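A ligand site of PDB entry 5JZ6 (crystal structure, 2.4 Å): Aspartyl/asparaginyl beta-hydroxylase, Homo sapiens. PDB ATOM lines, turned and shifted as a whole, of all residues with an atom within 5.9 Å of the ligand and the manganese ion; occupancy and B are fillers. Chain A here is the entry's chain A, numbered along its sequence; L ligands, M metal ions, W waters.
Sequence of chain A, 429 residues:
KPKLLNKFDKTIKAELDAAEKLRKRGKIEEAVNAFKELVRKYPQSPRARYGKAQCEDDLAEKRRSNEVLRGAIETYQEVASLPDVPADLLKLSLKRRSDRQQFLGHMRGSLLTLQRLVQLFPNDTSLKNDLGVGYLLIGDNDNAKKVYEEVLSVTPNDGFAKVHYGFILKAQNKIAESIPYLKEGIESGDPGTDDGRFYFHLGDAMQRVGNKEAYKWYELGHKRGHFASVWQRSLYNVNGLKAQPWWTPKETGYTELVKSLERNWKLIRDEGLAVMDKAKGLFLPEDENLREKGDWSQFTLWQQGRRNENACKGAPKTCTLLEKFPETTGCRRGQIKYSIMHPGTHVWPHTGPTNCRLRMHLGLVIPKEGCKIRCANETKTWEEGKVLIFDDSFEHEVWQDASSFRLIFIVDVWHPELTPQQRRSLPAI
The manganese ion is bound by water W1, 1.9 Å away. A ring nitrogen (NE2) of His 396 is bound to the manganese ion, at 2.2 Å. The manganese ion is bound by water W2, 2.2 Å away. O1 of the ligand is bound to the manganese ion, 2.2 Å away. O2 of the ligand is bound to the manganese ion (2.2 Å). NE2 of His 350 binds the manganese ion, at 2.3 Å. The manganese ion has six donor atoms within binding distance.
OG of Ser 339 lies within hydrogen-bond range of O4 of the ligand (2.7 Å). An oxygen (O3) of the ligand lies within hydrogen-bond range of a ring nitrogen (NE2) of His 361 (2.8 Å). O2 of the ligand lies close to NH1 of Arg 359 (2.8 Å). An oxygen (O5) of the ligand lies within salt-bridge range of the guanidinium group of Arg 406, 3.0 Å away. An oxygen (O4) of the ligand is in hydrogen-bond range of the indole nitrogen (NE1) of Trp 296 (3.2 Å).
The backbone carbonyl oxygen (O) of Ser 339 sits at hydrogen-bond distance from the guanidinium group (NH2) of Arg 406, at 3.2 Å. The indole nitrogen (NE1) of Trp 296 lies within hydrogen-bond range of the side-chain hydroxyl (OG) of Ser 339. The backbone NH (N) of Ser 339 is in hydrogen-bond range of the backbone carbonyl oxygen (O) of Ile 408 (3.0 Å). The indole nitrogen (NE1) of Trp 382 is in hydrogen-bond range of a ring nitrogen (ND1) of His 361, at 3.1 Å. N of Arg 359 lies within hydrogen-bond range of O of Phe 390 (2.9 Å). The side-chain carboxylate (OD2) of Asp 392 lies within salt-bridge range of the guanidinium group (NH1) of Arg 359, 3.9 Å away. O of Met 341 lies within hydrogen-bond range of N of Arg 406 (2.8 Å).
Two residues have an atom within 4 Å of the manganese ion: His 350 and His 396.
CE of Met 341 touches O4 of the ligand (3.7 Å). CD1 of Ile 408 touches O5 of the ligand, 3.7 Å away. CD1 of Ile 410 touches O3 of the ligand, at 3.4 Å. Hydrophobic or aromatic side chains within 4 Å of the ligand: Trp 296, Met 341, His 350, His 361, His 396, Ile 408 and Ile 410.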
ATOM      1  N   LEU A 290     -26.680  26.666   1.474  1.00  0.00           N
ATOM      2  CA  LEU A 290     -26.569  25.499   2.350  1.00  0.00           C
ATOM      3  C   LEU A 290     -25.195  24.841   2.265  1.00  0.00           C
ATOM      4  O   LEU A 290     -24.823  24.056   3.145  1.00  0.00           O
ATOM      5  CB  LEU A 290     -27.658  24.491   2.014  1.00  0.00           C
ATOM      6  CG  LEU A 290     -29.109  24.964   2.185  1.00  0.00           C
ATOM      7  CD1 LEU A 290     -30.073  23.862   1.787  1.00  0.00           C
ATOM      8  CD2 LEU A 290     -29.377  25.419   3.616  1.00  0.00           C
ATOM      9  N   TRP A 296     -21.442  19.784  -4.902  1.00  0.00           N
ATOM     10  CA  TRP A 296     -22.730  19.208  -4.577  1.00  0.00           C
ATOM     11  C   TRP A 296     -23.755  19.564  -5.647  1.00  0.00           C
ATOM     12  O   TRP A 296     -24.135  20.725  -5.785  1.00  0.00           O
ATOM     13  CB  TRP A 296     -23.172  19.705  -3.210  1.00  0.00           C
ATOM     14  CG  TRP A 296     -24.478  19.182  -2.729  1.00  0.00           C
ATOM     15  CD1 TRP A 296     -25.039  17.967  -2.999  1.00  0.00           C
ATOM     16  CD2 TRP A 296     -25.407  19.877  -1.880  1.00  0.00           C
ATOM     17  NE1 TRP A 296     -26.256  17.861  -2.365  1.00  0.00           N
ATOM     18  CE2 TRP A 296     -26.505  19.016  -1.674  1.00  0.00           C
ATOM     19  CE3 TRP A 296     -25.416  21.134  -1.272  1.00  0.00           C
ATOM     20  CZ2 TRP A 296     -27.594  19.377  -0.883  1.00  0.00           C
ATOM     21  CZ3 TRP A 296     -26.500  21.488  -0.492  1.00  0.00           C
ATOM     22  CH2 TRP A 296     -27.572  20.613  -0.310  1.00  0.00           C
ATOM     23  N   SER A 339     -28.616  13.030  -6.642  1.00  0.00           N
ATOM     24  CA  SER A 339     -27.799  13.978  -5.913  1.00  0.00           C
ATOM     25  C   SER A 339     -26.390  13.446  -5.736  1.00  0.00           C
ATOM     26  O   SER A 339     -26.181  12.390  -5.134  1.00  0.00           O
ATOM     27  CB  SER A 339     -28.425  14.289  -4.556  1.00  0.00           C
ATOM     28  OG  SER A 339     -27.643  15.216  -3.823  1.00  0.00           O
ATOM     29  N   ILE A 340     -25.411  14.171  -6.283  1.00  0.00           N
ATOM     30  CA  ILE A 340     -24.017  13.776  -6.180  1.00  0.00           C
ATOM     31  C   ILE A 340     -23.263  14.727  -5.250  1.00  0.00           C
ATOM     32  O   ILE A 340     -23.361  15.944  -5.378  1.00  0.00           O
ATOM     33  CB  ILE A 340     -23.347  13.706  -7.567  1.00  0.00           C
ATOM     34  CG1 ILE A 340     -21.889  13.280  -7.414  1.00  0.00           C
ATOM     35  CG2 ILE A 340     -23.437  15.045  -8.279  1.00  0.00           C
ATOM     36  CD1 ILE A 340     -21.278  12.762  -8.695  1.00  0.00           C
ATOM     37  N   MET A 341     -22.501  14.150  -4.330  1.00  0.00           N
ATOM     38  CA  MET A 341     -21.707  14.915  -3.392  1.00  0.00           C
ATOM     39  C   MET A 341     -20.275  14.395  -3.400  1.00  0.00           C
ATOM     40  O   MET A 341     -20.035  13.210  -3.242  1.00  0.00           O
ATOM     41  CB  MET A 341     -22.321  14.814  -1.989  1.00  0.00           C
ATOM     42  CG  MET A 341     -21.830  15.870  -1.016  1.00  0.00           C
ATOM     43  SD  MET A 341     -22.740  15.864   0.546  1.00  0.00           S
ATOM     44  CE  MET A 341     -24.352  16.419   0.015  1.00  0.00           C
ATOM     45  N   VAL A 347     -22.737  20.273   4.279  1.00  0.00           N
ATOM     46  CA  VAL A 347     -23.996  20.984   4.126  1.00  0.00           C
ATOM     47  C   VAL A 347     -24.437  21.495   5.493  1.00  0.00           C
ATOM     48  O   VAL A 347     -24.593  20.715   6.432  1.00  0.00           O
ATOM     49  CB  VAL A 347     -25.083  20.069   3.500  1.00  0.00           C
ATOM     50  CG1 VAL A 347     -26.377  20.839   3.293  1.00  0.00           C
ATOM     51  CG2 VAL A 347     -24.593  19.484   2.184  1.00  0.00           C
ATOM     52  N   HIS A 350     -30.105  22.422   8.432  1.00  0.00           N
ATOM     53  CA  HIS A 350     -31.254  23.113   7.867  1.00  0.00           C
ATOM     54  C   HIS A 350     -32.481  22.205   7.879  1.00  0.00           C
ATOM     55  O   HIS A 350     -32.368  21.005   8.147  1.00  0.00           O
ATOM     56  CB  HIS A 350     -30.958  23.556   6.431  1.00  0.00           C
ATOM     57  CG  HIS A 350     -30.849  22.427   5.468  1.00  0.00           C
ATOM     58  ND1 HIS A 350     -29.735  21.621   5.387  1.00  0.00           N
ATOM     59  CD2 HIS A 350     -31.727  21.953   4.551  1.00  0.00           C
ATOM     60  CE1 HIS A 350     -29.925  20.704   4.455  1.00  0.00           C
ATOM     61  NE2 HIS A 350     -31.115  20.879   3.930  1.00  0.00           N
ATOM     62  N   THR A 351     -33.637  22.775   7.574  1.00  0.00           N
ATOM     63  CA  THR A 351     -34.859  22.014   7.408  1.00  0.00           C
ATOM     64  C   THR A 351     -35.465  22.303   6.040  1.00  0.00           C
ATOM     65  O   THR A 351     -35.143  23.310   5.408  1.00  0.00           O
ATOM     66  CB  THR A 351     -35.917  22.337   8.506  1.00  0.00           C
ATOM     67  OG1 THR A 351     -36.514  23.620   8.243  1.00  0.00           O
ATOM     68  CG2 THR A 351     -35.287  22.358   9.890  1.00  0.00           C
ATOM     69  N   GLY A 352     -36.347  21.413   5.587  1.00  0.00           N
ATOM     70  CA  GLY A 352     -37.115  21.659   4.384  1.00  0.00           C
ATOM     71  C   GLY A 352     -38.252  22.630   4.666  1.00  0.00           C
ATOM     72  O   GLY A 352     -38.443  23.041   5.811  1.00  0.00           O
ATOM     73  N   ARG A 359     -38.768  12.181   3.058  1.00  0.00           N
ATOM     74  CA  ARG A 359     -37.701  12.109   2.077  1.00  0.00           C
ATOM     75  C   ARG A 359     -37.008  10.752   2.092  1.00  0.00           C
ATOM     76  O   ARG A 359     -36.436  10.340   3.106  1.00  0.00           O
ATOM     77  CB  ARG A 359     -36.677  13.220   2.345  1.00  0.00           C
ATOM     78  CG  ARG A 359     -35.489  13.200   1.399  1.00  0.00           C
ATOM     79  CD  ARG A 359     -34.934  14.593   1.169  1.00  0.00           C
ATOM     80  NE  ARG A 359     -35.766  15.377   0.266  1.00  0.00           N
ATOM     81  CZ  ARG A 359     -35.443  16.592  -0.197  1.00  0.00           C
ATOM     82  NH1 ARG A 359     -34.308  17.166   0.178  1.00  0.00           N
ATOM     83  NH2 ARG A 359     -36.260  17.225  -1.016  1.00  0.00           N
ATOM     84  N   HIS A 361     -34.028   8.291   0.687  1.00  0.00           N
ATOM     85  CA  HIS A 361     -32.706   8.259   0.064  1.00  0.00           C
ATOM     86  C   HIS A 361     -32.326   6.830  -0.332  1.00  0.00           C
ATOM     87  O   HIS A 361     -32.202   5.967   0.532  1.00  0.00           O
ATOM     88  CB  HIS A 361     -31.642   8.818   1.017  1.00  0.00           C
ATOM     89  CG  HIS A 361     -31.587  10.316   1.057  1.00  0.00           C
ATOM     90  ND1 HIS A 361     -30.628  10.984   1.775  1.00  0.00           N
ATOM     91  CD2 HIS A 361     -32.374  11.252   0.487  1.00  0.00           C
ATOM     92  CE1 HIS A 361     -30.811  12.288   1.643  1.00  0.00           C
ATOM     93  NE2 HIS A 361     -31.867  12.480   0.866  1.00  0.00           N
ATOM     94  N   ILE A 373     -25.150  11.291   7.402  1.00  0.00           N
ATOM     95  CA  ILE A 373     -26.226  12.274   7.473  1.00  0.00           C
ATOM     96  C   ILE A 373     -26.878  12.224   8.854  1.00  0.00           C
ATOM     97  O   ILE A 373     -27.214  11.157   9.354  1.00  0.00           O
ATOM     98  CB  ILE A 373     -27.277  12.029   6.368  1.00  0.00           C
ATOM     99  CG1 ILE A 373     -28.447  12.991   6.523  1.00  0.00           C
ATOM    100  CG2 ILE A 373     -27.757  10.577   6.392  1.00  0.00           C
ATOM    101  CD1 ILE A 373     -29.376  13.029   5.327  1.00  0.00           C
ATOM    102  N   TRP A 382     -25.408   5.821   4.420  1.00  0.00           N
ATOM    103  CA  TRP A 382     -26.136   5.185   3.335  1.00  0.00           C
ATOM    104  C   TRP A 382     -25.591   3.799   3.027  1.00  0.00           C
ATOM    105  O   TRP A 382     -24.462   3.467   3.404  1.00  0.00           O
ATOM    106  CB  TRP A 382     -26.077   6.040   2.069  1.00  0.00           C
ATOM    107  CG  TRP A 382     -26.710   7.383   2.217  1.00  0.00           C
ATOM    108  CD1 TRP A 382     -28.015   7.701   2.007  1.00  0.00           C
ATOM    109  CD2 TRP A 382     -26.049   8.593   2.583  1.00  0.00           C
ATOM    110  NE1 TRP A 382     -28.215   9.037   2.232  1.00  0.00           N
ATOM    111  CE2 TRP A 382     -27.025   9.611   2.590  1.00  0.00           C
ATOM    112  CE3 TRP A 382     -24.731   8.930   2.924  1.00  0.00           C
ATOM    113  CZ2 TRP A 382     -26.718  10.938   2.911  1.00  0.00           C
ATOM    114  CZ3 TRP A 382     -24.440  10.244   3.236  1.00  0.00           C
ATOM    115  CH2 TRP A 382     -25.426  11.226   3.233  1.00  0.00           C
ATOM    116  N   PHE A 390     -36.256   9.802   6.157  1.00  0.00           N
ATOM    117  CA  PHE A 390     -36.336  10.772   7.242  1.00  0.00           C
ATOM    118  C   PHE A 390     -37.283  11.918   6.905  1.00  0.00           C
ATOM    119  O   PHE A 390     -37.608  12.158   5.747  1.00  0.00           O
ATOM    120  CB  PHE A 390     -34.937  11.326   7.568  1.00  0.00           C
ATOM    121  CG  PHE A 390     -34.331  12.154   6.472  1.00  0.00           C
ATOM    122  CD1 PHE A 390     -33.759  11.569   5.367  1.00  0.00           C
ATOM    123  CD2 PHE A 390     -34.313  13.538   6.575  1.00  0.00           C
ATOM    124  CE1 PHE A 390     -33.191  12.332   4.366  1.00  0.00           C
ATOM    125  CE2 PHE A 390     -33.737  14.308   5.574  1.00  0.00           C
ATOM    126  CZ  PHE A 390     -33.173  13.701   4.468  1.00  0.00           C
ATOM    127  N   ASP A 392     -37.555  15.593   6.579  1.00  0.00           N
ATOM    128  CA  ASP A 392     -36.573  16.648   6.386  1.00  0.00           C
ATOM    129  C   ASP A 392     -37.099  18.007   6.863  1.00  0.00           C
ATOM    130  O   ASP A 392     -36.440  19.035   6.666  1.00  0.00           O
ATOM    131  CB  ASP A 392     -36.132  16.720   4.927  1.00  0.00           C
ATOM    132  CG  ASP A 392     -37.096  17.485   4.053  1.00  0.00           C
ATOM    133  OD1 ASP A 392     -38.319  17.378   4.263  1.00  0.00           O
ATOM    134  OD2 ASP A 392     -36.620  18.213   3.156  1.00  0.00           O
ATOM    135  N   HIS A 396     -31.525  18.607   9.561  1.00  0.00           N
ATOM    136  CA  HIS A 396     -30.575  17.581   9.134  1.00  0.00           C
ATOM    137  C   HIS A 396     -29.298  18.213   8.589  1.00  0.00           C
ATOM    138  O   HIS A 396     -29.300  19.364   8.162  1.00  0.00           O
ATOM    139  CB  HIS A 396     -31.218  16.659   8.087  1.00  0.00           C
ATOM    140  CG  HIS A 396     -31.831  17.388   6.937  1.00  0.00           C
ATOM    141  ND1 HIS A 396     -33.002  18.110   7.034  1.00  0.00           N
ATOM    142  CD2 HIS A 396     -31.438  17.485   5.638  1.00  0.00           C
ATOM    143  CE1 HIS A 396     -33.295  18.633   5.861  1.00  0.00           C
ATOM    144  NE2 HIS A 396     -32.367  18.271   4.993  1.00  0.00           N
ATOM    145  N   VAL A 398     -25.267  17.191   6.580  1.00  0.00           N
ATOM    146  CA  VAL A 398     -24.600  16.192   5.740  1.00  0.00           C
ATOM    147  C   VAL A 398     -23.103  16.445   5.626  1.00  0.00           C
ATOM    148  O   VAL A 398     -22.666  17.597   5.497  1.00  0.00           O
ATOM    149  CB  VAL A 398     -25.255  16.150   4.339  1.00  0.00           C
ATOM    150  CG1 VAL A 398     -24.654  15.033   3.505  1.00  0.00           C
ATOM    151  CG2 VAL A 398     -26.772  15.962   4.458  1.00  0.00           C
ATOM    152  N   ARG A 406     -20.152  10.465  -3.931  1.00  0.00           N
ATOM    153  CA  ARG A 406     -21.316   9.808  -3.343  1.00  0.00           C
ATOM    154  C   ARG A 406     -22.553  10.141  -4.160  1.00  0.00           C
ATOM    155  O   ARG A 406     -22.907  11.301  -4.312  1.00  0.00           O
ATOM    156  CB  ARG A 406     -21.502  10.239  -1.885  1.00  0.00           C
ATOM    157  CG  ARG A 406     -22.670   9.571  -1.177  1.00  0.00           C
ATOM    158  CD  ARG A 406     -23.577  10.596  -0.512  1.00  0.00           C
ATOM    159  NE  ARG A 406     -24.254  11.456  -1.486  1.00  0.00           N
ATOM    160  CZ  ARG A 406     -25.076  12.452  -1.159  1.00  0.00           C
ATOM    161  NH1 ARG A 406     -25.337  12.720   0.112  1.00  0.00           N
ATOM    162  NH2 ARG A 406     -25.639  13.167  -2.114  1.00  0.00           N
ATOM    163  N   ILE A 408     -26.689   9.398  -4.680  1.00  0.00           N
ATOM    164  CA  ILE A 408     -27.923   8.884  -4.098  1.00  0.00           C
ATOM    165  C   ILE A 408     -29.108   9.287  -4.960  1.00  0.00           C
ATOM    166  O   ILE A 408     -29.026  10.221  -5.751  1.00  0.00           O
ATOM    167  CB  ILE A 408     -28.123   9.372  -2.646  1.00  0.00           C
ATOM    168  CG1 ILE A 408     -28.240  10.902  -2.609  1.00  0.00           C
ATOM    169  CG2 ILE A 408     -26.980   8.884  -1.770  1.00  0.00           C
ATOM    170  CD1 ILE A 408     -28.610  11.454  -1.252  1.00  0.00           C
ATOM    171  N   ILE A 410     -33.011  10.566  -4.620  1.00  0.00           N
ATOM    172  CA  ILE A 410     -33.871  11.205  -3.631  1.00  0.00           C
ATOM    173  C   ILE A 410     -35.315  11.158  -4.095  1.00  0.00           C
ATOM    174  O   ILE A 410     -35.636  11.588  -5.207  1.00  0.00           O
ATOM    175  CB  ILE A 410     -33.418  12.664  -3.358  1.00  0.00           C
ATOM    176  CG1 ILE A 410     -31.969  12.667  -2.856  1.00  0.00           C
ATOM    177  CG2 ILE A 410     -34.346  13.332  -2.349  1.00  0.00           C
ATOM    178  CD1 ILE A 410     -31.402  14.037  -2.572  1.00  0.00           C
HETATM  179  C1  LIG L   1     -30.834  16.954   2.061  1.00  0.00           C
HETATM  180  O1  LIG L   1     -30.242  17.751   2.838  1.00  0.00           O
HETATM  181  O2  LIG L   1     -32.068  17.108   1.825  1.00  0.00           O
HETATM  182  C2  LIG L   1     -30.073  15.820   1.395  1.00  0.00           C
HETATM  183  O3  LIG L   1     -30.954  15.089   0.592  1.00  0.00           O
HETATM  184  C3  LIG L   1     -28.953  16.388   0.528  1.00  0.00           C
HETATM  185  C4  LIG L   1     -28.030  15.257   0.080  1.00  0.00           C
HETATM  186  O4  LIG L   1     -27.624  15.209  -1.115  1.00  0.00           O
HETATM  187  O5  LIG L   1     -27.678  14.368   0.899  1.00  0.00           O
HETATM  188 MN    MN M   1     -32.038  19.042   2.966  1.00  0.00          MN
HETATM  189  O   HOH W   1     -33.798  19.707   2.906  1.00  0.00           O
HETATM  190  O   HOH W   2     -31.928  20.049   1.019  1.00  0.00           O
